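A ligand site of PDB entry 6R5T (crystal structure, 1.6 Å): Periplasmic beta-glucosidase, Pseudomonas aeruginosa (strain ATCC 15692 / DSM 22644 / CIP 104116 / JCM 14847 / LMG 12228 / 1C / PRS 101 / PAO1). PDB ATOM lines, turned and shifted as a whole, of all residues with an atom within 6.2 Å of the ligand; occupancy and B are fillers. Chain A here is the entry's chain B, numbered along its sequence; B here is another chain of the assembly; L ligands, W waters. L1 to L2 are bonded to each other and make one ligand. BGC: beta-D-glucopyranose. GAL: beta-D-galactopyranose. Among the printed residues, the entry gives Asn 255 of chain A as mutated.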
ATOM      1  N   PHE A  50     -21.458  42.331 -11.982  1.00  0.00           N
ATOM      2  CA  PHE A  50     -21.033  41.149 -11.204  1.00  0.00           C
ATOM      3  C   PHE A  50     -19.691  40.649 -11.746  1.00  0.00           C
ATOM      4  O   PHE A  50     -19.366  40.904 -12.914  1.00  0.00           O
ATOM      5  CB  PHE A  50     -22.103  40.066 -11.174  1.00  0.00           C
ATOM      6  CG  PHE A  50     -22.443  39.398 -12.482  1.00  0.00           C
ATOM      7  CD1 PHE A  50     -23.228  40.045 -13.424  1.00  0.00           C
ATOM      8  CD2 PHE A  50     -21.982  38.124 -12.780  1.00  0.00           C
ATOM      9  CE1 PHE A  50     -23.577  39.468 -14.611  1.00  0.00           C
ATOM     10  CE2 PHE A  50     -22.302  37.554 -14.009  1.00  0.00           C
ATOM     11  CZ  PHE A  50     -23.106  38.202 -14.916  1.00  0.00           C
ATOM     12  N   ASN A  51     -18.972  39.942 -10.880  1.00  0.00           N
ATOM     13  CA  ASN A  51     -17.693  39.242 -11.182  1.00  0.00           C
ATOM     14  C   ASN A  51     -16.524  40.209 -11.311  1.00  0.00           C
ATOM     15  O   ASN A  51     -15.456  39.727 -11.714  1.00  0.00           O
ATOM     16  CB  ASN A  51     -17.833  38.366 -12.430  1.00  0.00           C
ATOM     17  CG  ASN A  51     -18.559  37.047 -12.191  1.00  0.00           C
ATOM     18  OD1 ASN A  51     -18.851  36.704 -11.065  1.00  0.00           O
ATOM     19  ND2 ASN A  51     -18.902  36.360 -13.272  1.00  0.00           N
ATOM     20  N   ASP A  79     -20.500  35.850  -6.343  1.00  0.00           N
ATOM     21  CA  ASP A  79     -20.956  34.519  -5.830  1.00  0.00           C
ATOM     22  C   ASP A  79     -20.053  34.180  -4.643  1.00  0.00           C
ATOM     23  O   ASP A  79     -19.176  33.350  -4.746  1.00  0.00           O
ATOM     24  CB  ASP A  79     -20.910  33.513  -6.973  1.00  0.00           C
ATOM     25  CG  ASP A  79     -22.059  33.659  -7.958  1.00  0.00           C
ATOM     26  OD1 ASP A  79     -23.232  33.563  -7.496  1.00  0.00           O
ATOM     27  OD2 ASP A  79     -21.822  33.831  -9.185  1.00  0.00           O
ATOM     28  N   PHE A 123     -24.589  36.758  -4.255  1.00  0.00           N
ATOM     29  CA  PHE A 123     -25.665  35.831  -4.683  1.00  0.00           C
ATOM     30  C   PHE A 123     -25.608  34.615  -3.759  1.00  0.00           C
ATOM     31  O   PHE A 123     -25.045  33.580  -4.124  1.00  0.00           O
ATOM     32  CB  PHE A 123     -25.439  35.473  -6.139  1.00  0.00           C
ATOM     33  CG  PHE A 123     -25.400  36.644  -7.090  1.00  0.00           C
ATOM     34  CD1 PHE A 123     -26.347  37.648  -7.033  1.00  0.00           C
ATOM     35  CD2 PHE A 123     -24.428  36.708  -8.052  1.00  0.00           C
ATOM     36  CE1 PHE A 123     -26.284  38.701  -7.944  1.00  0.00           C
ATOM     37  CE2 PHE A 123     -24.363  37.763  -8.941  1.00  0.00           C
ATOM     38  CZ  PHE A 123     -25.303  38.731  -8.886  1.00  0.00           C
ATOM     39  N   ARG A 137     -25.525  20.448  -7.666  1.00  0.00           N
ATOM     40  CA  ARG A 137     -25.579  21.641  -6.786  1.00  0.00           C
ATOM     41  C   ARG A 137     -25.999  21.325  -5.369  1.00  0.00           C
ATOM     42  O   ARG A 137     -26.192  22.261  -4.563  1.00  0.00           O
ATOM     43  CB  ARG A 137     -26.460  22.686  -7.453  1.00  0.00           C
ATOM     44  CG  ARG A 137     -25.977  23.028  -8.845  1.00  0.00           C
ATOM     45  CD  ARG A 137     -26.666  24.236  -9.489  1.00  0.00           C
ATOM     46  NE  ARG A 137     -26.117  25.433  -8.860  1.00  0.00           N
ATOM     47  CZ  ARG A 137     -26.023  26.629  -9.437  1.00  0.00           C
ATOM     48  NH1 ARG A 137     -26.486  26.821 -10.659  1.00  0.00           N
ATOM     49  NH2 ARG A 137     -25.416  27.611  -8.770  1.00  0.00           N
ATOM     50  N   GLU A 140     -24.056  23.091  -2.638  1.00  0.00           N
ATOM     51  CA  GLU A 140     -24.326  24.528  -2.353  1.00  0.00           C
ATOM     52  C   GLU A 140     -25.409  24.747  -1.326  1.00  0.00           C
ATOM     53  O   GLU A 140     -25.492  25.870  -0.852  1.00  0.00           O
ATOM     54  CB  GLU A 140     -24.780  25.223  -3.626  1.00  0.00           C
ATOM     55  CG  GLU A 140     -23.677  25.301  -4.596  1.00  0.00           C
ATOM     56  CD  GLU A 140     -24.232  25.683  -5.933  1.00  0.00           C
ATOM     57  OE1 GLU A 140     -24.928  26.759  -5.990  1.00  0.00           O
ATOM     58  OE2 GLU A 140     -23.987  24.860  -6.875  1.00  0.00           O
ATOM     59  N   LYS A 176     -31.141  32.655  -3.072  1.00  0.00           N
ATOM     60  CA  LYS A 176     -31.313  31.937  -4.373  1.00  0.00           C
ATOM     61  C   LYS A 176     -31.614  30.463  -4.054  1.00  0.00           C
ATOM     62  O   LYS A 176     -31.361  30.024  -2.931  1.00  0.00           O
ATOM     63  CB  LYS A 176     -30.070  32.106  -5.233  1.00  0.00           C
ATOM     64  CG  LYS A 176     -28.814  31.395  -4.763  1.00  0.00           C
ATOM     65  CD  LYS A 176     -27.595  31.775  -5.555  1.00  0.00           C
ATOM     66  CE  LYS A 176     -26.370  30.991  -5.237  1.00  0.00           C
ATOM     67  NZ  LYS A 176     -25.210  31.535  -6.000  1.00  0.00           N
ATOM     68  N   HIS A 177     -32.167  29.700  -4.986  1.00  0.00           N
ATOM     69  CA  HIS A 177     -32.613  30.076  -6.328  1.00  0.00           C
ATOM     70  C   HIS A 177     -34.151  29.998  -6.303  1.00  0.00           C
ATOM     71  O   HIS A 177     -34.686  28.896  -6.159  1.00  0.00           O
ATOM     72  CB  HIS A 177     -32.048  29.136  -7.375  1.00  0.00           C
ATOM     73  CG  HIS A 177     -30.560  29.065  -7.431  1.00  0.00           C
ATOM     74  ND1 HIS A 177     -29.860  28.133  -6.692  1.00  0.00           N
ATOM     75  CD2 HIS A 177     -29.670  29.768  -8.167  1.00  0.00           C
ATOM     76  CE1 HIS A 177     -28.568  28.292  -7.012  1.00  0.00           C
ATOM     77  NE2 HIS A 177     -28.427  29.274  -7.860  1.00  0.00           N
ATOM     78  N   TYR A 181     -35.424  24.818  -7.286  1.00  0.00           N
ATOM     79  CA  TYR A 181     -34.411  24.439  -8.288  1.00  0.00           C
ATOM     80  C   TYR A 181     -33.815  23.058  -7.990  1.00  0.00           C
ATOM     81  O   TYR A 181     -33.505  22.299  -8.920  1.00  0.00           O
ATOM     82  CB  TYR A 181     -33.367  25.556  -8.266  1.00  0.00           C
ATOM     83  CG  TYR A 181     -32.225  25.449  -9.226  1.00  0.00           C
ATOM     84  CD1 TYR A 181     -32.340  25.011 -10.533  1.00  0.00           C
ATOM     85  CD2 TYR A 181     -30.990  25.863  -8.789  1.00  0.00           C
ATOM     86  CE1 TYR A 181     -31.212  24.925 -11.351  1.00  0.00           C
ATOM     87  CE2 TYR A 181     -29.878  25.841  -9.600  1.00  0.00           C
ATOM     88  CZ  TYR A 181     -29.985  25.339 -10.877  1.00  0.00           C
ATOM     89  OH  TYR A 181     -28.853  25.296 -11.664  1.00  0.00           O
ATOM     90  N   ASP A 189     -29.363  18.931 -13.896  1.00  0.00           N
ATOM     91  CA  ASP A 189     -29.433  20.380 -13.634  1.00  0.00           C
ATOM     92  C   ASP A 189     -30.341  21.051 -14.677  1.00  0.00           C
ATOM     93  O   ASP A 189     -30.451  20.613 -15.854  1.00  0.00           O
ATOM     94  CB  ASP A 189     -28.030  20.985 -13.571  1.00  0.00           C
ATOM     95  CG  ASP A 189     -27.969  22.246 -12.708  1.00  0.00           C
ATOM     96  OD1 ASP A 189     -29.045  22.736 -12.239  1.00  0.00           O
ATOM     97  OD2 ASP A 189     -26.818  22.712 -12.453  1.00  0.00           O
ATOM     98  N   TYR A 190     -31.022  22.088 -14.222  1.00  0.00           N
ATOM     99  CA  TYR A 190     -31.909  22.947 -15.030  1.00  0.00           C
ATOM    100  C   TYR A 190     -33.201  22.219 -15.404  1.00  0.00           C
ATOM    101  O   TYR A 190     -34.066  22.857 -16.036  1.00  0.00           O
ATOM    102  CB  TYR A 190     -31.206  23.379 -16.306  1.00  0.00           C
ATOM    103  CG  TYR A 190     -29.771  23.798 -16.161  1.00  0.00           C
ATOM    104  CD1 TYR A 190     -29.385  24.800 -15.275  1.00  0.00           C
ATOM    105  CD2 TYR A 190     -28.815  23.181 -16.945  1.00  0.00           C
ATOM    106  CE1 TYR A 190     -28.064  25.210 -15.223  1.00  0.00           C
ATOM    107  CE2 TYR A 190     -27.495  23.577 -16.896  1.00  0.00           C
ATOM    108  CZ  TYR A 190     -27.121  24.557 -16.007  1.00  0.00           C
ATOM    109  OH  TYR A 190     -25.798  25.021 -16.002  1.00  0.00           O
ATOM    110  N   MET A 220     -32.721  36.044  -6.107  1.00  0.00           N
ATOM    111  CA  MET A 220     -32.276  35.594  -7.436  1.00  0.00           C
ATOM    112  C   MET A 220     -33.234  34.493  -7.904  1.00  0.00           C
ATOM    113  O   MET A 220     -33.421  33.503  -7.180  1.00  0.00           O
ATOM    114  CB  MET A 220     -30.834  35.097  -7.452  1.00  0.00           C
ATOM    115  CG  MET A 220     -30.478  34.683  -8.822  1.00  0.00           C
ATOM    116  SD  MET A 220     -28.782  34.141  -8.948  1.00  0.00           S
ATOM    117  CE  MET A 220     -28.066  35.732  -9.374  1.00  0.00           C
ATOM    118  N   LEU A 223     -33.723  28.966 -12.684  1.00  0.00           N
ATOM    119  CA  LEU A 223     -33.693  28.662 -14.124  1.00  0.00           C
ATOM    120  C   LEU A 223     -34.735  27.627 -14.533  1.00  0.00           C
ATOM    121  O   LEU A 223     -34.890  27.455 -15.746  1.00  0.00           O
ATOM    122  CB  LEU A 223     -32.294  28.142 -14.455  1.00  0.00           C
ATOM    123  CG  LEU A 223     -31.166  29.179 -14.460  1.00  0.00           C
ATOM    124  CD1 LEU A 223     -29.822  28.425 -14.529  1.00  0.00           C
ATOM    125  CD2 LEU A 223     -31.290  30.110 -15.625  1.00  0.00           C
ATOM    126  N   ASN A 255     -31.672  35.150 -13.303  1.00  0.00           N
ATOM    127  CA  ASN A 255     -30.452  34.374 -13.432  1.00  0.00           C
ATOM    128  C   ASN A 255     -29.809  34.681 -14.777  1.00  0.00           C
ATOM    129  O   ASN A 255     -30.302  35.470 -15.631  1.00  0.00           O
ATOM    130  CB  ASN A 255     -30.827  32.908 -13.196  1.00  0.00           C
ATOM    131  CG  ASN A 255     -29.822  32.156 -12.382  1.00  0.00           C
ATOM    132  OD1 ASN A 255     -28.665  32.130 -12.775  1.00  0.00           O
ATOM    133  ND2 ASN A 255     -30.292  31.547 -11.273  1.00  0.00           N
ATOM    134  N   HIS A 256     -28.740  33.988 -15.044  1.00  0.00           N
ATOM    135  CA  HIS A 256     -27.790  34.383 -16.087  1.00  0.00           C
ATOM    136  C   HIS A 256     -28.324  34.006 -17.473  1.00  0.00           C
ATOM    137  O   HIS A 256     -28.439  32.811 -17.742  1.00  0.00           O
ATOM    138  CB  HIS A 256     -26.475  33.715 -15.732  1.00  0.00           C
ATOM    139  CG  HIS A 256     -25.394  34.188 -16.609  1.00  0.00           C
ATOM    140  ND1 HIS A 256     -25.360  33.917 -17.964  1.00  0.00           N
ATOM    141  CD2 HIS A 256     -24.314  34.950 -16.325  1.00  0.00           C
ATOM    142  CE1 HIS A 256     -24.298  34.512 -18.489  1.00  0.00           C
ATOM    143  NE2 HIS A 256     -23.633  35.116 -17.498  1.00  0.00           N
ATOM    144  N   MET A 287     -29.973  39.914 -15.913  1.00  0.00           N
ATOM    145  CA  MET A 287     -28.544  39.475 -15.859  1.00  0.00           C
ATOM    146  C   MET A 287     -28.068  39.070 -17.244  1.00  0.00           C
ATOM    147  O   MET A 287     -28.583  38.091 -17.848  1.00  0.00           O
ATOM    148  CB  MET A 287     -28.355  38.378 -14.818  1.00  0.00           C
ATOM    149  CG  MET A 287     -26.948  37.971 -14.568  1.00  0.00           C
ATOM    150  SD  MET A 287     -26.966  36.744 -13.189  1.00  0.00           S
ATOM    151  CE  MET A 287     -25.475  37.144 -12.298  1.00  0.00           C
ATOM    152  N   TRP A 398     -17.710  26.629  -6.339  1.00  0.00           N
ATOM    153  CA  TRP A 398     -18.153  28.018  -6.009  1.00  0.00           C
ATOM    154  C   TRP A 398     -17.208  28.565  -4.943  1.00  0.00           C
ATOM    155  O   TRP A 398     -17.652  29.027  -3.872  1.00  0.00           O
ATOM    156  CB  TRP A 398     -19.628  28.081  -5.615  1.00  0.00           C
ATOM    157  CG  TRP A 398     -20.572  27.764  -6.769  1.00  0.00           C
ATOM    158  CD1 TRP A 398     -21.339  26.635  -6.900  1.00  0.00           C
ATOM    159  CD2 TRP A 398     -20.884  28.562  -7.929  1.00  0.00           C
ATOM    160  NE1 TRP A 398     -22.023  26.657  -8.103  1.00  0.00           N
ATOM    161  CE2 TRP A 398     -21.791  27.840  -8.729  1.00  0.00           C
ATOM    162  CE3 TRP A 398     -20.480  29.831  -8.374  1.00  0.00           C
ATOM    163  CZ2 TRP A 398     -22.294  28.337  -9.942  1.00  0.00           C
ATOM    164  CZ3 TRP A 398     -20.954  30.310  -9.577  1.00  0.00           C
ATOM    165  CH2 TRP A 398     -21.840  29.575 -10.359  1.00  0.00           C
ATOM    166  N   GLU A 486     -22.264  23.152 -10.652  1.00  0.00           N
ATOM    167  CA  GLU A 486     -23.327  23.396 -11.646  1.00  0.00           C
ATOM    168  C   GLU A 486     -23.179  22.451 -12.837  1.00  0.00           C
ATOM    169  O   GLU A 486     -22.056  22.289 -13.403  1.00  0.00           O
ATOM    170  CB  GLU A 486     -23.291  24.855 -12.079  1.00  0.00           C
ATOM    171  CG  GLU A 486     -24.285  25.151 -13.172  1.00  0.00           C
ATOM    172  CD  GLU A 486     -24.284  26.561 -13.665  1.00  0.00           C
ATOM    173  OE1 GLU A 486     -23.414  27.350 -13.168  1.00  0.00           O
ATOM    174  OE2 GLU A 486     -25.212  26.935 -14.468  1.00  0.00           O
ATOM    175  N   ARG B 585     -31.863  25.078 -21.099  1.00  0.00           N
ATOM    176  CA  ARG B 585     -30.454  24.733 -21.472  1.00  0.00           C
ATOM    177  C   ARG B 585     -30.441  23.301 -21.968  1.00  0.00           C
ATOM    178  O   ARG B 585     -29.783  22.435 -21.388  1.00  0.00           O
ATOM    179  CB  ARG B 585     -29.496  24.944 -20.298  1.00  0.00           C
ATOM    180  CG  ARG B 585     -29.322  26.399 -19.939  1.00  0.00           C
ATOM    181  CD  ARG B 585     -28.403  26.626 -18.760  1.00  0.00           C
ATOM    182  NE  ARG B 585     -28.392  28.044 -18.412  1.00  0.00           N
ATOM    183  CZ  ARG B 585     -27.543  28.628 -17.590  1.00  0.00           C
ATOM    184  NH1 ARG B 585     -26.575  27.926 -17.032  1.00  0.00           N
ATOM    185  NH2 ARG B 585     -27.604  29.921 -17.347  1.00  0.00           N
ATOM    186  N   TYR B 595     -22.739  23.148 -19.953  1.00  0.00           N
ATOM    187  CA  TYR B 595     -23.788  23.900 -19.225  1.00  0.00           C
ATOM    188  C   TYR B 595     -25.142  23.624 -19.862  1.00  0.00           C
ATOM    189  O   TYR B 595     -25.869  24.555 -20.253  1.00  0.00           O
ATOM    190  CB  TYR B 595     -23.439  25.362 -19.027  1.00  0.00           C
ATOM    191  CG  TYR B 595     -22.226  25.497 -18.157  1.00  0.00           C
ATOM    192  CD1 TYR B 595     -22.353  25.393 -16.780  1.00  0.00           C
ATOM    193  CD2 TYR B 595     -20.952  25.651 -18.688  1.00  0.00           C
ATOM    194  CE1 TYR B 595     -21.263  25.514 -15.940  1.00  0.00           C
ATOM    195  CE2 TYR B 595     -19.843  25.743 -17.854  1.00  0.00           C
ATOM    196  CZ  TYR B 595     -20.001  25.649 -16.482  1.00  0.00           C
ATOM    197  OH  TYR B 595     -18.943  25.711 -15.624  1.00  0.00           O
HETATM  198  C2  BGC L   1     -25.084  32.261  -9.615  1.00  0.00           C
HETATM  199  C3  BGC L   1     -24.967  32.977 -10.969  1.00  0.00           C
HETATM  200  C4  BGC L   1     -24.552  31.877 -11.996  1.00  0.00           C
HETATM  201  C5  BGC L   1     -25.690  30.834 -11.999  1.00  0.00           C
HETATM  202  C6  BGC L   1     -25.396  29.659 -12.909  1.00  0.00           C
HETATM  203  C1  BGC L   1     -26.112  31.124  -9.721  1.00  0.00           C
HETATM  204  O1  BGC L   1     -26.048  30.480  -8.486  1.00  0.00           O
HETATM  205  O2  BGC L   1     -25.484  33.104  -8.543  1.00  0.00           O
HETATM  206  O3  BGC L   1     -23.920  33.966 -10.888  1.00  0.00           O
HETATM  207  O4  BGC L   1     -24.438  32.497 -13.276  1.00  0.00           O
HETATM  208  O5  BGC L   1     -25.724  30.215 -10.750  1.00  0.00           O
HETATM  209  O6  BGC L   1     -26.505  28.757 -12.898  1.00  0.00           O
HETATM  210  C1  GAL L   2     -23.164  32.407 -13.924  1.00  0.00           C
HETATM  211  C2  GAL L   2     -22.048  33.122 -13.123  1.00  0.00           C
HETATM  212  C3  GAL L   2     -20.759  33.031 -13.938  1.00  0.00           C
HETATM  213  C4  GAL L   2     -20.451  31.525 -14.182  1.00  0.00           C
HETATM  214  C5  GAL L   2     -21.669  30.879 -14.865  1.00  0.00           C
HETATM  215  C6  GAL L   2     -21.489  29.369 -15.012  1.00  0.00           C
HETATM  216  O2  GAL L   2     -22.427  34.474 -12.918  1.00  0.00           O
HETATM  217  O3  GAL L   2     -19.701  33.624 -13.161  1.00  0.00           O
HETATM  218  O4  GAL L   2     -20.238  30.975 -12.865  1.00  0.00           O
HETATM  219  O5  GAL L   2     -22.895  31.025 -14.054  1.00  0.00           O
HETATM  220  O6  GAL L   2     -22.698  28.808 -15.583  1.00  0.00           O
HETATM  221  O   HOH W   1     -24.792  30.458 -16.477  1.00  0.00           O
HETATM  222  O   HOH W   2     -28.724  29.179 -11.223  1.00  0.00           O
HETATM  223  O   HOH W   3     -19.357  33.809 -10.301  1.00  0.00           O
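O2 of BGC L1 is in hydrogen-bond range of OD1 of Asp 79 (2.5 Å). O6 of BGC L1 lies within hydrogen-bond range of OE2 of Glu 486, 2.7 Å away. NE2 of His 177 lies within hydrogen-bond range of O1 of BGC L1. The side-chain amino group (NZ) of Lys 176 sits at hydrogen-bond distance from an oxygen (O1) of BGC L1, 2.8 Å away. ND2 of Asn 51 is in hydrogen-bond range of O3 of GAL L2. The guanidinium group (NH2) of Arg 137 sits at hydrogen-bond distance from an oxygen (O1) of BGC L1, 3.0 Å away. An oxygen (O2) of BGC L1 sits at hydrogen-bond distance from the side-chain sulfur of Met 220 (3.5 Å).
Water W1 bridges O6 of GAL L2 and NH2 of Arg 585 of chain B. Water W2 lies within hydrogen-bond range of an oxygen (O6) of BGC L1 (2.8 Å), the side-chain amide nitrogen of Asn 255 (2.8 Å), the guanidinium group of Arg 137 (3.3 Å) and a ring nitrogen (NE2) of His 177 (3.4 Å). Water W3 lies within hydrogen-bond range of the side-chain carboxylate (OD2) of Asp 79 (2.7 Å), an oxygen (O3) of GAL L2 (2.9 Å) and the side-chain amide oxygen (OD1) of Asn 51 (3.0 Å).
OD1 of Asp 79 is in salt-bridge range of NZ of Lys 176 (3.2 Å). The side-chain hydroxyl (OH) of Tyr 190 is in hydrogen-bond range of the side-chain carboxylate (OE2) of Glu 486, at 2.5 Å. NZ of Lys 176 lies within hydrogen-bond range of O of Phe 123. NH1 of Arg 137 sits at hydrogen-bond distance from OH of Tyr 181 (3.0 Å). The indole nitrogen (NE1) of Trp 398 is in hydrogen-bond range of the side-chain carboxylate (OE2) of Glu 140. The side-chain amide nitrogen (ND2) of Asn 255 is in hydrogen-bond range of the side-chain sulfur (SD) of Met 220, at 3.8 Å. The side-chain sulfur (SD) of Met 287 lies within hydrogen-bond range of the backbone NH (N) of His 256 (3.8 Å). O of His 256 sits at hydrogen-bond distance from NH2 of Arg 585 of chain B (3.0 Å).
CE2 of Phe 50 touches O2 of GAL L2, 3.3 Å away. Phe 123 touches the ligand. CD1 of Leu 223 touches O6 of BGC L1, 3.7 Å away. OD1 of Asn 255 touches C5 of BGC L1 (3.3 Å). His 256 touches the ligand. Met 287 touches the ligand. Trp 398 touches the ligand. Tyr 595 of chain B touches the ligand. Hydrophobic or aromatic side chains that line the ligand: Phe 50, Phe 123, His 177, Met 220, Leu 223, His 256, Met 287, Trp 398 and Tyr 595 of chain B. 15 residues have an atom within 4 Å of the ligand: Phe 50, Asn 51, Asp 79, Phe 123, Arg 137, Lys 176, His 177, Met 220, Leu 223, Asn 255, His 256, Met 287, Trp 398, Glu 486 and Tyr 595 of chain B. The nearest printed residue that does not touch the ligand is Arg 585 of chain B (4.2 Å).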
